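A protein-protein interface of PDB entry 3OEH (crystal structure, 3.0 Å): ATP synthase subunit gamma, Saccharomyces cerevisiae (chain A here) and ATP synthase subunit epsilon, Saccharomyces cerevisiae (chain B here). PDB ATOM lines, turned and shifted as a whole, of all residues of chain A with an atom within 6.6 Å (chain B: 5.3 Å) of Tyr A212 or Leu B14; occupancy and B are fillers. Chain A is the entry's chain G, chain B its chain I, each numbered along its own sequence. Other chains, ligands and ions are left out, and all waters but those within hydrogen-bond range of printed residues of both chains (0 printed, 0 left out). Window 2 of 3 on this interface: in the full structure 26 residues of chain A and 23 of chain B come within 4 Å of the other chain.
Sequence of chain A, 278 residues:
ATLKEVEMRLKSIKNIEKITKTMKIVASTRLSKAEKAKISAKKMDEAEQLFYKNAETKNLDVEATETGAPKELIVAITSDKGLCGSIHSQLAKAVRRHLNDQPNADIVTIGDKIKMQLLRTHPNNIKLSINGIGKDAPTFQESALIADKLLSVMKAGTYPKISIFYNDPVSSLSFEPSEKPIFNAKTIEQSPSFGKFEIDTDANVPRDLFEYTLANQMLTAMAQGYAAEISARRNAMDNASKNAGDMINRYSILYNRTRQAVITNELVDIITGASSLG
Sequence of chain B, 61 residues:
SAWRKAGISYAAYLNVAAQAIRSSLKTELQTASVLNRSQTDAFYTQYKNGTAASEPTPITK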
ATOM      1  N   MET A  44      21.223  29.683 -13.974  1.00  0.00           N
ATOM      2  CA  MET A  44      21.110  28.502 -14.822  1.00  0.00           C
ATOM      3  C   MET A  44      19.869  28.529 -15.713  1.00  0.00           C
ATOM      4  O   MET A  44      19.789  27.779 -16.694  1.00  0.00           O
ATOM      5  CB  MET A  44      21.097  27.237 -13.974  1.00  0.00           C
ATOM      6  CG  MET A  44      21.510  26.001 -14.728  1.00  0.00           C
ATOM      7  SD  MET A  44      20.649  24.578 -14.083  1.00  0.00           S
ATOM      8  CE  MET A  44      21.792  23.287 -14.560  1.00  0.00           C
ATOM      9  N   GLU A  48      19.700  27.912 -19.940  1.00  0.00           N
ATOM     10  CA  GLU A  48      18.888  26.811 -20.440  1.00  0.00           C
ATOM     11  C   GLU A  48      17.684  27.281 -21.259  1.00  0.00           C
ATOM     12  O   GLU A  48      17.379  26.710 -22.305  1.00  0.00           O
ATOM     13  CB  GLU A  48      18.444  25.917 -19.280  1.00  0.00           C
ATOM     14  CG  GLU A  48      16.963  25.593 -19.279  1.00  0.00           C
ATOM     15  CD  GLU A  48      16.677  24.211 -18.765  1.00  0.00           C
ATOM     16  OE1 GLU A  48      17.114  23.233 -19.417  1.00  0.00           O
ATOM     17  OE2 GLU A  48      16.003  24.106 -17.714  1.00  0.00           O
ATOM     18  N   TYR A  52      15.400  28.133 -26.025  1.00  0.00           N
ATOM     19  CA  TYR A  52      13.979  28.264 -26.367  1.00  0.00           C
ATOM     20  C   TYR A  52      13.615  29.665 -26.850  1.00  0.00           C
ATOM     21  O   TYR A  52      12.759  29.814 -27.722  1.00  0.00           O
ATOM     22  CB  TYR A  52      13.097  27.905 -25.173  1.00  0.00           C
ATOM     23  CG  TYR A  52      13.231  26.483 -24.687  1.00  0.00           C
ATOM     24  CD1 TYR A  52      14.104  26.166 -23.649  1.00  0.00           C
ATOM     25  CD2 TYR A  52      12.475  25.457 -25.256  1.00  0.00           C
ATOM     26  CE1 TYR A  52      14.230  24.870 -23.192  1.00  0.00           C
ATOM     27  CE2 TYR A  52      12.593  24.151 -24.801  1.00  0.00           C
ATOM     28  CZ  TYR A  52      13.475  23.869 -23.768  1.00  0.00           C
ATOM     29  OH  TYR A  52      13.605  22.581 -23.310  1.00  0.00           O
ATOM     30  N   PHE A 140      17.942  19.150  -7.238  1.00  0.00           N
ATOM     31  CA  PHE A 140      17.733  18.443  -8.490  1.00  0.00           C
ATOM     32  C   PHE A 140      17.208  17.015  -8.283  1.00  0.00           C
ATOM     33  O   PHE A 140      16.419  16.529  -9.084  1.00  0.00           O
ATOM     34  CB  PHE A 140      19.022  18.441  -9.321  1.00  0.00           C
ATOM     35  CG  PHE A 140      18.810  18.097 -10.773  1.00  0.00           C
ATOM     36  CD1 PHE A 140      18.767  16.767 -11.191  1.00  0.00           C
ATOM     37  CD2 PHE A 140      18.649  19.102 -11.723  1.00  0.00           C
ATOM     38  CE1 PHE A 140      18.559  16.447 -12.518  1.00  0.00           C
ATOM     39  CE2 PHE A 140      18.443  18.790 -13.057  1.00  0.00           C
ATOM     40  CZ  PHE A 140      18.400  17.459 -13.453  1.00  0.00           C
ATOM     41  N   ARG A 207      13.031  15.065 -27.073  1.00  0.00           N
ATOM     42  CA  ARG A 207      12.558  14.232 -25.950  1.00  0.00           C
ATOM     43  C   ARG A 207      13.394  14.420 -24.684  1.00  0.00           C
ATOM     44  O   ARG A 207      12.851  14.611 -23.600  1.00  0.00           O
ATOM     45  CB  ARG A 207      12.525  12.757 -26.341  1.00  0.00           C
ATOM     46  CG  ARG A 207      12.339  11.795 -25.176  1.00  0.00           C
ATOM     47  CD  ARG A 207      13.083  10.493 -25.437  1.00  0.00           C
ATOM     48  NE  ARG A 207      12.809   9.490 -24.411  1.00  0.00           N
ATOM     49  CZ  ARG A 207      11.817   8.602 -24.464  1.00  0.00           C
ATOM     50  NH1 ARG A 207      10.984   8.581 -25.500  1.00  0.00           N
ATOM     51  NH2 ARG A 207      11.657   7.733 -23.473  1.00  0.00           N
ATOM     52  N   ASP A 208      14.715  14.361 -24.836  1.00  0.00           N
ATOM     53  CA  ASP A 208      15.633  14.553 -23.720  1.00  0.00           C
ATOM     54  C   ASP A 208      15.590  15.977 -23.235  1.00  0.00           C
ATOM     55  O   ASP A 208      15.553  16.225 -22.034  1.00  0.00           O
ATOM     56  CB  ASP A 208      17.057  14.187 -24.122  1.00  0.00           C
ATOM     57  CG  ASP A 208      17.256  12.691 -24.262  1.00  0.00           C
ATOM     58  OD1 ASP A 208      16.388  11.912 -23.800  1.00  0.00           O
ATOM     59  OD2 ASP A 208      18.288  12.290 -24.838  1.00  0.00           O
ATOM     60  N   LEU A 209      15.576  16.913 -24.177  1.00  0.00           N
ATOM     61  CA  LEU A 209      15.488  18.330 -23.855  1.00  0.00           C
ATOM     62  C   LEU A 209      14.238  18.655 -23.040  1.00  0.00           C
ATOM     63  O   LEU A 209      14.264  19.529 -22.187  1.00  0.00           O
ATOM     64  CB  LEU A 209      15.550  19.169 -25.127  1.00  0.00           C
ATOM     65  CG  LEU A 209      16.184  20.558 -25.054  1.00  0.00           C
ATOM     66  CD1 LEU A 209      17.238  20.680 -23.951  1.00  0.00           C
ATOM     67  CD2 LEU A 209      16.770  20.935 -26.420  1.00  0.00           C
ATOM     68  N   PHE A 210      13.153  17.931 -23.287  1.00  0.00           N
ATOM     69  CA  PHE A 210      11.929  18.112 -22.523  1.00  0.00           C
ATOM     70  C   PHE A 210      12.028  17.544 -21.113  1.00  0.00           C
ATOM     71  O   PHE A 210      11.715  18.245 -20.155  1.00  0.00           O
ATOM     72  CB  PHE A 210      10.731  17.522 -23.270  1.00  0.00           C
ATOM     73  CG  PHE A 210       9.566  17.166 -22.388  1.00  0.00           C
ATOM     74  CD1 PHE A 210       8.861  18.146 -21.696  1.00  0.00           C
ATOM     75  CD2 PHE A 210       9.157  15.844 -22.273  1.00  0.00           C
ATOM     76  CE1 PHE A 210       7.778  17.805 -20.889  1.00  0.00           C
ATOM     77  CE2 PHE A 210       8.078  15.501 -21.471  1.00  0.00           C
ATOM     78  CZ  PHE A 210       7.387  16.481 -20.784  1.00  0.00           C
ATOM     79  N   GLU A 211      12.460  16.290 -20.982  1.00  0.00           N
ATOM     80  CA  GLU A 211      12.539  15.642 -19.667  1.00  0.00           C
ATOM     81  C   GLU A 211      13.564  16.311 -18.756  1.00  0.00           C
ATOM     82  O   GLU A 211      13.392  16.370 -17.539  1.00  0.00           O
ATOM     83  CB  GLU A 211      12.858  14.161 -19.808  1.00  0.00           C
ATOM     84  CG  GLU A 211      11.874  13.408 -20.678  1.00  0.00           C
ATOM     85  CD  GLU A 211      12.027  11.906 -20.585  1.00  0.00           C
ATOM     86  OE1 GLU A 211      12.891  11.426 -19.815  1.00  0.00           O
ATOM     87  OE2 GLU A 211      11.267  11.206 -21.286  1.00  0.00           O
ATOM     88  N   TYR A 212      14.629  16.815 -19.366  1.00  0.00           N
ATOM     89  CA  TYR A 212      15.627  17.588 -18.660  1.00  0.00           C
ATOM     90  C   TYR A 212      15.016  18.906 -18.184  1.00  0.00           C
ATOM     91  O   TYR A 212      15.161  19.269 -17.021  1.00  0.00           O
ATOM     92  CB  TYR A 212      16.838  17.818 -19.564  1.00  0.00           C
ATOM     93  CG  TYR A 212      17.990  18.555 -18.924  1.00  0.00           C
ATOM     94  CD1 TYR A 212      18.854  17.908 -18.041  1.00  0.00           C
ATOM     95  CD2 TYR A 212      18.232  19.897 -19.222  1.00  0.00           C
ATOM     96  CE1 TYR A 212      19.921  18.581 -17.457  1.00  0.00           C
ATOM     97  CE2 TYR A 212      19.296  20.579 -18.646  1.00  0.00           C
ATOM     98  CZ  TYR A 212      20.135  19.917 -17.762  1.00  0.00           C
ATOM     99  OH  TYR A 212      21.186  20.591 -17.183  1.00  0.00           O
ATOM    100  N   THR A 213      14.309  19.604 -19.069  1.00  0.00           N
ATOM    101  CA  THR A 213      13.717  20.900 -18.710  1.00  0.00           C
ATOM    102  C   THR A 213      12.513  20.780 -17.759  1.00  0.00           C
ATOM    103  O   THR A 213      12.217  21.723 -17.014  1.00  0.00           O
ATOM    104  CB  THR A 213      13.364  21.764 -19.945  1.00  0.00           C
ATOM    105  OG1 THR A 213      14.462  21.761 -20.861  1.00  0.00           O
ATOM    106  CG2 THR A 213      13.109  23.211 -19.531  1.00  0.00           C
ATOM    107  N   LEU A 214      11.833  19.632 -17.775  1.00  0.00           N
ATOM    108  CA  LEU A 214      10.806  19.358 -16.770  1.00  0.00           C
ATOM    109  C   LEU A 214      11.465  19.401 -15.400  1.00  0.00           C
ATOM    110  O   LEU A 214      11.118  20.232 -14.567  1.00  0.00           O
ATOM    111  CB  LEU A 214      10.128  18.006 -17.000  1.00  0.00           C
ATOM    112  CG  LEU A 214       8.836  17.726 -16.222  1.00  0.00           C
ATOM    113  CD1 LEU A 214       7.773  18.803 -16.457  1.00  0.00           C
ATOM    114  CD2 LEU A 214       8.290  16.351 -16.565  1.00  0.00           C
ATOM    115  N   ALA A 215      12.441  18.520 -15.191  1.00  0.00           N
ATOM    116  CA  ALA A 215      13.217  18.492 -13.958  1.00  0.00           C
ATOM    117  C   ALA A 215      13.808  19.857 -13.659  1.00  0.00           C
ATOM    118  O   ALA A 215      13.580  20.409 -12.599  1.00  0.00           O
ATOM    119  CB  ALA A 215      14.305  17.457 -14.050  1.00  0.00           C
ATOM    120  N   ASN A 216      14.527  20.414 -14.620  1.00  0.00           N
ATOM    121  CA  ASN A 216      15.345  21.600 -14.392  1.00  0.00           C
ATOM    122  C   ASN A 216      14.578  22.871 -14.042  1.00  0.00           C
ATOM    123  O   ASN A 216      14.986  23.622 -13.168  1.00  0.00           O
ATOM    124  CB  ASN A 216      16.248  21.841 -15.601  1.00  0.00           C
ATOM    125  CG  ASN A 216      17.603  22.384 -15.217  1.00  0.00           C
ATOM    126  OD1 ASN A 216      18.071  23.352 -15.806  1.00  0.00           O
ATOM    127  ND2 ASN A 216      18.249  21.761 -14.226  1.00  0.00           N
ATOM    128  N   GLN A 217      13.468  23.112 -14.720  1.00  0.00           N
ATOM    129  CA  GLN A 217      12.717  24.342 -14.494  1.00  0.00           C
ATOM    130  C   GLN A 217      11.764  24.263 -13.302  1.00  0.00           C
ATOM    131  O   GLN A 217      11.332  25.283 -12.755  1.00  0.00           O
ATOM    132  CB  GLN A 217      12.006  24.778 -15.763  1.00  0.00           C
ATOM    133  CG  GLN A 217      12.880  25.647 -16.620  1.00  0.00           C
ATOM    134  CD  GLN A 217      12.102  26.775 -17.234  1.00  0.00           C
ATOM    135  OE1 GLN A 217      12.332  27.937 -16.912  1.00  0.00           O
ATOM    136  NE2 GLN A 217      11.151  26.444 -18.107  1.00  0.00           N
ATOM    137  N   SER B   9      14.542   7.700 -16.718  1.00  0.00           N
ATOM    138  CA  SER B   9      14.160   8.837 -17.562  1.00  0.00           C
ATOM    139  C   SER B   9      15.270   9.874 -17.477  1.00  0.00           C
ATOM    140  O   SER B   9      15.852  10.043 -16.413  1.00  0.00           O
ATOM    141  CB  SER B   9      12.857   9.459 -17.070  1.00  0.00           C
ATOM    142  OG  SER B   9      13.024   9.999 -15.769  1.00  0.00           O
ATOM    143  N   TYR B  10      15.540  10.583 -18.574  1.00  0.00           N
ATOM    144  CA  TYR B  10      16.737  11.438 -18.686  1.00  0.00           C
ATOM    145  C   TYR B  10      17.086  12.266 -17.431  1.00  0.00           C
ATOM    146  O   TYR B  10      18.261  12.496 -17.148  1.00  0.00           O
ATOM    147  CB  TYR B  10      16.683  12.331 -19.942  1.00  0.00           C
ATOM    148  CG  TYR B  10      17.994  13.056 -20.231  1.00  0.00           C
ATOM    149  CD1 TYR B  10      19.015  12.438 -20.962  1.00  0.00           C
ATOM    150  CD2 TYR B  10      18.217  14.354 -19.762  1.00  0.00           C
ATOM    151  CE1 TYR B  10      20.228  13.098 -21.218  1.00  0.00           C
ATOM    152  CE2 TYR B  10      19.421  15.020 -20.014  1.00  0.00           C
ATOM    153  CZ  TYR B  10      20.425  14.391 -20.742  1.00  0.00           C
ATOM    154  OH  TYR B  10      21.616  15.055 -20.981  1.00  0.00           O
ATOM    155  N   ALA B  11      16.074  12.707 -16.690  1.00  0.00           N
ATOM    156  CA  ALA B  11      16.298  13.410 -15.431  1.00  0.00           C
ATOM    157  C   ALA B  11      16.764  12.431 -14.350  1.00  0.00           C
ATOM    158  O   ALA B  11      17.839  12.599 -13.762  1.00  0.00           O
ATOM    159  CB  ALA B  11      15.030  14.112 -15.002  1.00  0.00           C
ATOM    160  N   ALA B  12      15.945  11.409 -14.102  1.00  0.00           N
ATOM    161  CA  ALA B  12      16.248  10.340 -13.151  1.00  0.00           C
ATOM    162  C   ALA B  12      17.529   9.592 -13.520  1.00  0.00           C
ATOM    163  O   ALA B  12      18.170   8.987 -12.660  1.00  0.00           O
ATOM    164  CB  ALA B  12      15.073   9.369 -13.067  1.00  0.00           C
ATOM    165  N   TYR B  13      17.884   9.643 -14.802  1.00  0.00           N
ATOM    166  CA  TYR B  13      19.053   8.968 -15.361  1.00  0.00           C
ATOM    167  C   TYR B  13      20.343   9.742 -15.081  1.00  0.00           C
ATOM    168  O   TYR B  13      21.380   9.141 -14.820  1.00  0.00           O
ATOM    169  CB  TYR B  13      18.833   8.738 -16.868  1.00  0.00           C
ATOM    170  CG  TYR B  13      20.076   8.527 -17.705  1.00  0.00           C
ATOM    171  CD1 TYR B  13      20.631   9.579 -18.436  1.00  0.00           C
ATOM    172  CD2 TYR B  13      20.684   7.272 -17.787  1.00  0.00           C
ATOM    173  CE1 TYR B  13      21.769   9.397 -19.209  1.00  0.00           C
ATOM    174  CE2 TYR B  13      21.824   7.075 -18.561  1.00  0.00           C
ATOM    175  CZ  TYR B  13      22.362   8.144 -19.270  1.00  0.00           C
ATOM    176  OH  TYR B  13      23.488   7.961 -20.040  1.00  0.00           O
ATOM    177  N   LEU B  14      20.273  11.068 -15.132  1.00  0.00           N
ATOM    178  CA  LEU B  14      21.419  11.918 -14.802  1.00  0.00           C
ATOM    179  C   LEU B  14      21.599  12.023 -13.298  1.00  0.00           C
ATOM    180  O   LEU B  14      22.710  12.241 -12.815  1.00  0.00           O
ATOM    181  CB  LEU B  14      21.256  13.323 -15.388  1.00  0.00           C
ATOM    182  CG  LEU B  14      21.489  13.629 -16.871  1.00  0.00           C
ATOM    183  CD1 LEU B  14      21.560  15.132 -17.043  1.00  0.00           C
ATOM    184  CD2 LEU B  14      22.753  12.979 -17.423  1.00  0.00           C
ATOM    185  N   ASN B  15      20.492  11.881 -12.572  1.00  0.00           N
ATOM    186  CA  ASN B  15      20.487  11.907 -11.111  1.00  0.00           C
ATOM    187  C   ASN B  15      21.282  10.757 -10.490  1.00  0.00           C
ATOM    188  O   ASN B  15      22.093  10.975  -9.590  1.00  0.00           O
ATOM    189  CB  ASN B  15      19.048  11.903 -10.578  1.00  0.00           C
ATOM    190  CG  ASN B  15      18.982  11.710  -9.065  1.00  0.00           C
ATOM    191  OD1 ASN B  15      18.552  10.660  -8.581  1.00  0.00           O
ATOM    192  ND2 ASN B  15      19.424  12.718  -8.314  1.00  0.00           N
ATOM    193  N   VAL B  16      21.041   9.536 -10.969  1.00  0.00           N
ATOM    194  CA  VAL B  16      21.778   8.366 -10.490  1.00  0.00           C
ATOM    195  C   VAL B  16      23.272   8.521 -10.814  1.00  0.00           C
ATOM    196  O   VAL B  16      24.131   8.057 -10.059  1.00  0.00           O
ATOM    197  CB  VAL B  16      21.207   7.023 -11.044  1.00  0.00           C
ATOM    198  CG1 VAL B  16      21.720   5.835 -10.218  1.00  0.00           C
ATOM    199  CG2 VAL B  16      19.686   7.023 -11.020  1.00  0.00           C
ATOM    200  N   ALA B  17      23.572   9.199 -11.921  1.00  0.00           N
ATOM    201  CA  ALA B  17      24.947   9.585 -12.252  1.00  0.00           C
ATOM    202  C   ALA B  17      25.463  10.715 -11.349  1.00  0.00           C
ATOM    203  O   ALA B  17      26.673  10.904 -11.206  1.00  0.00           O
ATOM    204  CB  ALA B  17      25.054   9.985 -13.721  1.00  0.00           C
ATOM    205  N   ALA B  18      24.538  11.461 -10.744  1.00  0.00           N
ATOM    206  CA  ALA B  18      24.884  12.549  -9.828  1.00  0.00           C
ATOM    207  C   ALA B  18      25.003  12.042  -8.381  1.00  0.00           C
ATOM    208  O   ALA B  18      25.072  12.834  -7.428  1.00  0.00           O
ATOM    209  CB  ALA B  18      23.847  13.670  -9.936  1.00  0.00           C
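The backbone NH (N) of Tyr B10 lies within hydrogen-bond range of the side-chain carboxylate (OE1) of Glu A211, 3.0 Å away.
Tyr A212 touches just these residues of chain B: Tyr B10 (3.5 Å) and Leu B14 (3.8 Å). Of the printed residues of chain B, Ala A215 touches Ala B11 (3.6 Å). Printed residues of chain A within 4 Å of Ala B11: Glu A211 (3.8 Å) and Ala A215 (3.6 Å). Gln A217 touches none of the printed residues of chain B. The nearest residue of chain B that does not touch Tyr A212 is Ala B11 (5.1 Å). The nearest residue of chain A that does not touch Leu B14 is Phe A140 (5.0 Å).
The side-chain carboxylate (OE2) of Glu A211 lies within salt-bridge range of the guanidinium group (NE) of Arg A207 (3.9 Å).
Tyr B10 touches Asp A208 (CD1 to CG, 3.7 Å). CB of Ser B9 touches OE1 of Glu A211, 3.4 Å away. CB of Ala B11 touches O of Glu A211, at 3.8 Å. Tyr A212 touches Tyr B10. Tyr A212 touches Leu B14 (CE1 to CD1, 3.8 Å). Ala A215 touches Ala B11 (CB to CB, 3.6 Å).
Hydrophobic or aromatic side chains of chain A that line the printed part of chain B: Tyr A212 and Ala A215. Hydrophobic or aromatic side chains of chain B within 4 Å of the printed part of chain A: Tyr B10, Ala B11 and Leu B14. Among the printed residues, no Asp or Glu carboxylate lies within 4 Å of a Lys or Arg side-chain nitrogen of the other chain.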
